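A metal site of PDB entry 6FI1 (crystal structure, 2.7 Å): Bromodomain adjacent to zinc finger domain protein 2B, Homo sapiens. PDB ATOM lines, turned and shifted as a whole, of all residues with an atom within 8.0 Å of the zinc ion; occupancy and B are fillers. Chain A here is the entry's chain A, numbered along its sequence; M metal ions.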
ATOM      1  N   TYR A   8       5.849 -15.265  24.066  1.00  0.00           N
ATOM      2  CA  TYR A   8       5.892 -13.874  24.525  1.00  0.00           C
ATOM      3  C   TYR A   8       5.745 -13.850  26.050  1.00  0.00           C
ATOM      4  O   TYR A   8       5.088 -14.728  26.657  1.00  0.00           O
ATOM      5  CB  TYR A   8       4.792 -13.069  23.823  1.00  0.00           C
ATOM      6  CG  TYR A   8       5.020 -12.879  22.325  1.00  0.00           C
ATOM      7  CD1 TYR A   8       5.912 -11.929  21.840  1.00  0.00           C
ATOM      8  CD2 TYR A   8       4.340 -13.658  21.384  1.00  0.00           C
ATOM      9  CE1 TYR A   8       6.122 -11.741  20.489  1.00  0.00           C
ATOM     10  CE2 TYR A   8       4.536 -13.486  20.021  1.00  0.00           C
ATOM     11  CZ  TYR A   8       5.428 -12.523  19.571  1.00  0.00           C
ATOM     12  OH  TYR A   8       5.636 -12.342  18.225  1.00  0.00           O
ATOM     13  N   CYS A   9       6.331 -12.860  26.686  1.00  0.00           N
ATOM     14  CA  CYS A   9       6.292 -12.763  28.111  1.00  0.00           C
ATOM     15  C   CYS A   9       4.947 -12.236  28.489  1.00  0.00           C
ATOM     16  O   CYS A   9       4.523 -11.199  27.975  1.00  0.00           O
ATOM     17  CB  CYS A   9       7.409 -11.811  28.598  1.00  0.00           C
ATOM     18  SG  CYS A   9       7.087 -11.015  30.179  1.00  0.00           S
ATOM     19  N   GLN A  10       4.249 -12.924  29.388  1.00  0.00           N
ATOM     20  CA  GLN A  10       2.880 -12.509  29.777  1.00  0.00           C
ATOM     21  C   GLN A  10       2.775 -11.056  30.191  1.00  0.00           C
ATOM     22  O   GLN A  10       1.731 -10.516  30.087  1.00  0.00           O
ATOM     23  CB  GLN A  10       2.365 -13.305  30.965  1.00  0.00           C
ATOM     24  CG  GLN A  10       1.960 -14.723  30.704  1.00  0.00           C
ATOM     25  CD  GLN A  10       1.006 -14.831  29.540  1.00  0.00           C
ATOM     26  OE1 GLN A  10       1.442 -14.918  28.372  1.00  0.00           O
ATOM     27  NE2 GLN A  10      -0.305 -14.833  29.839  1.00  0.00           N
ATOM     28  N   ILE A  11       3.846 -10.466  30.708  1.00  0.00           N
ATOM     29  CA  ILE A  11       3.789  -9.125  31.266  1.00  0.00           C
ATOM     30  C   ILE A  11       4.099  -8.041  30.246  1.00  0.00           C
ATOM     31  O   ILE A  11       3.294  -7.180  29.980  1.00  0.00           O
ATOM     32  CB  ILE A  11       4.768  -9.014  32.445  1.00  0.00           C
ATOM     33  CG1 ILE A  11       4.492 -10.114  33.491  1.00  0.00           C
ATOM     34  CG2 ILE A  11       4.705  -7.648  33.086  1.00  0.00           C
ATOM     35  CD1 ILE A  11       3.117 -10.040  34.110  1.00  0.00           C
ATOM     36  N   CYS A  12       5.301  -8.047  29.701  1.00  0.00           N
ATOM     37  CA  CYS A  12       5.656  -6.988  28.770  1.00  0.00           C
ATOM     38  C   CYS A  12       5.213  -7.313  27.362  1.00  0.00           C
ATOM     39  O   CYS A  12       5.200  -6.449  26.502  1.00  0.00           O
ATOM     40  CB  CYS A  12       7.144  -6.730  28.816  1.00  0.00           C
ATOM     41  SG  CYS A  12       8.024  -8.157  28.263  1.00  0.00           S
ATOM     42  N   ARG A  13       4.865  -8.578  27.123  1.00  0.00           N
ATOM     43  CA  ARG A  13       4.253  -9.032  25.870  1.00  0.00           C
ATOM     44  C   ARG A  13       5.232  -9.040  24.700  1.00  0.00           C
ATOM     45  O   ARG A  13       4.857  -8.789  23.560  1.00  0.00           O
ATOM     46  CB  ARG A  13       2.998  -8.212  25.558  1.00  0.00           C
ATOM     47  CG  ARG A  13       2.036  -7.993  26.726  1.00  0.00           C
ATOM     48  CD  ARG A  13       1.328  -9.262  27.183  1.00  0.00           C
ATOM     49  NE  ARG A  13       0.510  -9.874  26.135  1.00  0.00           N
ATOM     50  CZ  ARG A  13      -0.269 -10.936  26.307  1.00  0.00           C
ATOM     51  NH1 ARG A  13      -0.355 -11.536  27.517  1.00  0.00           N
ATOM     52  NH2 ARG A  13      -0.965 -11.428  25.281  1.00  0.00           N
ATOM     53  N   LYS A  14       6.476  -9.387  24.989  1.00  0.00           N
ATOM     54  CA  LYS A  14       7.557  -9.413  24.024  1.00  0.00           C
ATOM     55  C   LYS A  14       8.360 -10.673  24.200  1.00  0.00           C
ATOM     56  O   LYS A  14       8.532 -11.146  25.322  1.00  0.00           O
ATOM     57  CB  LYS A  14       8.513  -8.235  24.234  1.00  0.00           C
ATOM     58  CG  LYS A  14       7.904  -6.844  24.173  1.00  0.00           C
ATOM     59  CD  LYS A  14       8.838  -5.829  24.809  1.00  0.00           C
ATOM     60  CE  LYS A  14      10.255  -5.897  24.216  1.00  0.00           C
ATOM     61  NZ  LYS A  14      10.992  -4.605  24.389  1.00  0.00           N
ATOM     62  N   GLY A  15       8.878 -11.195  23.102  1.00  0.00           N
ATOM     63  CA  GLY A  15       9.609 -12.460  23.087  1.00  0.00           C
ATOM     64  C   GLY A  15      11.118 -12.298  23.083  1.00  0.00           C
ATOM     65  O   GLY A  15      11.828 -13.291  22.995  1.00  0.00           O
ATOM     66  N   ASP A  16      11.619 -11.067  23.233  1.00  0.00           N
ATOM     67  CA  ASP A  16      13.066 -10.838  23.276  1.00  0.00           C
ATOM     68  C   ASP A  16      13.720 -11.376  24.571  1.00  0.00           C
ATOM     69  O   ASP A  16      13.065 -11.897  25.435  1.00  0.00           O
ATOM     70  CB  ASP A  16      13.351  -9.352  23.114  1.00  0.00           C
ATOM     71  CG  ASP A  16      13.097  -8.583  24.376  1.00  0.00           C
ATOM     72  OD1 ASP A  16      12.195  -9.006  25.118  1.00  0.00           O
ATOM     73  OD2 ASP A  16      13.793  -7.566  24.626  1.00  0.00           O
ATOM     74  N   ASN A  17      15.029 -11.240  24.710  1.00  0.00           N
ATOM     75  CA  ASN A  17      15.775 -11.778  25.852  1.00  0.00           C
ATOM     76  C   ASN A  17      15.441 -13.209  26.257  1.00  0.00           C
ATOM     77  O   ASN A  17      15.442 -13.541  27.431  1.00  0.00           O
ATOM     78  CB  ASN A  17      15.663 -10.852  27.054  1.00  0.00           C
ATOM     79  CG  ASN A  17      16.194  -9.470  26.765  1.00  0.00           C
ATOM     80  OD1 ASN A  17      15.429  -8.505  26.776  1.00  0.00           O
ATOM     81  ND2 ASN A  17      17.507  -9.368  26.497  1.00  0.00           N
ATOM     82  N   LEU A  20      16.448 -14.903  29.501  1.00  0.00           N
ATOM     83  CA  LEU A  20      15.775 -14.580  30.769  1.00  0.00           C
ATOM     84  C   LEU A  20      14.277 -14.826  30.736  1.00  0.00           C
ATOM     85  O   LEU A  20      13.541 -14.318  31.574  1.00  0.00           O
ATOM     86  CB  LEU A  20      16.051 -13.123  31.117  1.00  0.00           C
ATOM     87  CG  LEU A  20      17.491 -12.695  31.356  1.00  0.00           C
ATOM     88  CD1 LEU A  20      17.463 -11.210  31.655  1.00  0.00           C
ATOM     89  CD2 LEU A  20      18.184 -13.457  32.486  1.00  0.00           C
ATOM     90  N   LEU A  21      13.819 -15.616  29.781  1.00  0.00           N
ATOM     91  CA  LEU A  21      12.416 -15.824  29.562  1.00  0.00           C
ATOM     92  C   LEU A  21      12.058 -17.171  30.121  1.00  0.00           C
ATOM     93  O   LEU A  21      12.471 -18.185  29.594  1.00  0.00           O
ATOM     94  CB  LEU A  21      12.088 -15.731  28.073  1.00  0.00           C
ATOM     95  CG  LEU A  21      10.603 -15.657  27.646  1.00  0.00           C
ATOM     96  CD1 LEU A  21       9.748 -14.560  28.299  1.00  0.00           C
ATOM     97  CD2 LEU A  21      10.529 -15.462  26.139  1.00  0.00           C
ATOM     98  N   GLY A  30       5.042 -17.792  29.392  1.00  0.00           N
ATOM     99  CA  GLY A  30       6.359 -17.207  29.483  1.00  0.00           C
ATOM    100  C   GLY A  30       6.281 -16.004  30.364  1.00  0.00           C
ATOM    101  O   GLY A  30       5.237 -15.401  30.499  1.00  0.00           O
ATOM    102  N   CYS A  31       7.381 -15.723  31.028  1.00  0.00           N
ATOM    103  CA  CYS A  31       7.530 -14.504  31.763  1.00  0.00           C
ATOM    104  C   CYS A  31       9.033 -14.198  31.948  1.00  0.00           C
ATOM    105  O   CYS A  31       9.773 -15.021  32.412  1.00  0.00           O
ATOM    106  CB  CYS A  31       6.830 -14.605  33.105  1.00  0.00           C
ATOM    107  SG  CYS A  31       6.709 -12.980  33.814  1.00  0.00           S
ATOM    108  N   HIS A  32       9.465 -13.024  31.563  1.00  0.00           N
ATOM    109  CA  HIS A  32      10.852 -12.598  31.813  1.00  0.00           C
ATOM    110  C   HIS A  32      11.091 -12.563  33.301  1.00  0.00           C
ATOM    111  O   HIS A  32      10.202 -12.165  34.067  1.00  0.00           O
ATOM    112  CB  HIS A  32      11.097 -11.187  31.345  1.00  0.00           C
ATOM    113  CG  HIS A  32      11.064 -11.036  29.880  1.00  0.00           C
ATOM    114  ND1 HIS A  32      10.232 -10.137  29.257  1.00  0.00           N
ATOM    115  CD2 HIS A  32      11.796 -11.626  28.913  1.00  0.00           C
ATOM    116  CE1 HIS A  32      10.438 -10.203  27.958  1.00  0.00           C
ATOM    117  NE2 HIS A  32      11.399 -11.089  27.718  1.00  0.00           N
ATOM    118  N   THR A  33      12.295 -12.943  33.702  1.00  0.00           N
ATOM    119  CA  THR A  33      12.669 -12.909  35.104  1.00  0.00           C
ATOM    120  C   THR A  33      12.500 -11.480  35.650  1.00  0.00           C
ATOM    121  O   THR A  33      12.077 -11.245  36.780  1.00  0.00           O
ATOM    122  CB  THR A  33      14.144 -13.328  35.302  1.00  0.00           C
ATOM    123  OG1 THR A  33      14.958 -12.661  34.353  1.00  0.00           O
ATOM    124  CG2 THR A  33      14.347 -14.780  35.135  1.00  0.00           C
ATOM    125  N   TYR A  34      12.897 -10.517  34.829  1.00  0.00           N
ATOM    126  CA  TYR A  34      12.875  -9.108  35.235  1.00  0.00           C
ATOM    127  C   TYR A  34      11.440  -8.511  35.257  1.00  0.00           C
ATOM    128  O   TYR A  34      11.222  -7.459  35.862  1.00  0.00           O
ATOM    129  CB  TYR A  34      13.836  -8.281  34.352  1.00  0.00           C
ATOM    130  CG  TYR A  34      13.601  -8.344  32.846  1.00  0.00           C
ATOM    131  CD1 TYR A  34      12.650  -7.524  32.226  1.00  0.00           C
ATOM    132  CD2 TYR A  34      14.314  -9.230  32.042  1.00  0.00           C
ATOM    133  CE1 TYR A  34      12.433  -7.575  30.881  1.00  0.00           C
ATOM    134  CE2 TYR A  34      14.106  -9.293  30.667  1.00  0.00           C
ATOM    135  CZ  TYR A  34      13.170  -8.465  30.098  1.00  0.00           C
ATOM    136  OH  TYR A  34      12.961  -8.506  28.717  1.00  0.00           O
ATOM    137  N   CYS A  35      10.488  -9.154  34.596  1.00  0.00           N
ATOM    138  CA  CYS A  35       9.084  -8.747  34.634  1.00  0.00           C
ATOM    139  C   CYS A  35       8.339  -9.268  35.842  1.00  0.00           C
ATOM    140  O   CYS A  35       7.337  -8.704  36.269  1.00  0.00           O
ATOM    141  CB  CYS A  35       8.370  -9.138  33.340  1.00  0.00           C
ATOM    142  SG  CYS A  35       8.890  -8.076  31.978  1.00  0.00           S
ATOM    143  N   HIS A  36       8.823 -10.353  36.385  1.00  0.00           N
ATOM    144  CA  HIS A  36       8.286 -10.910  37.610  1.00  0.00           C
ATOM    145  C   HIS A  36       8.367  -9.942  38.773  1.00  0.00           C
ATOM    146  O   HIS A  36       9.383  -9.225  38.921  1.00  0.00           O
ATOM    147  CB  HIS A  36       9.089 -12.156  37.978  1.00  0.00           C
ATOM    148  CG  HIS A  36       8.223 -13.285  38.387  1.00  0.00           C
ATOM    149  ND1 HIS A  36       7.821 -13.469  39.685  1.00  0.00           N
ATOM    150  CD2 HIS A  36       7.633 -14.244  37.654  1.00  0.00           C
ATOM    151  CE1 HIS A  36       7.039 -14.527  39.742  1.00  0.00           C
ATOM    152  NE2 HIS A  36       6.920 -15.026  38.523  1.00  0.00           N
HETATM  153 ZN    ZN M   1       8.691  -9.375  30.097  1.00  0.00          ZN
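NE2 of His 32 lies within hydrogen-bond range of O of Asp 16 (2.9 Å). A ring nitrogen (NE2) of His 32 lies close to the side-chain hydroxyl (OH) of Tyr 34, 3.2 Å away. SG of Cys 9 lies close to N of Ile 11 (3.3 Å). The backbone NH (N) of Cys 9 sits at hydrogen-bond distance from the backbone carbonyl oxygen (O) of Lys 14.
Four residues have an atom within 4 Å of the zinc ion: Cys 9, Cys 12, His 32 and Cys 35.
The zinc ion is bound by ND1 of His 32 (1.9 Å), SG of Cys 35 (2.3 Å), SG of Cys 9 (2.3 Å) and SG of Cys 12 (2.3 Å).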
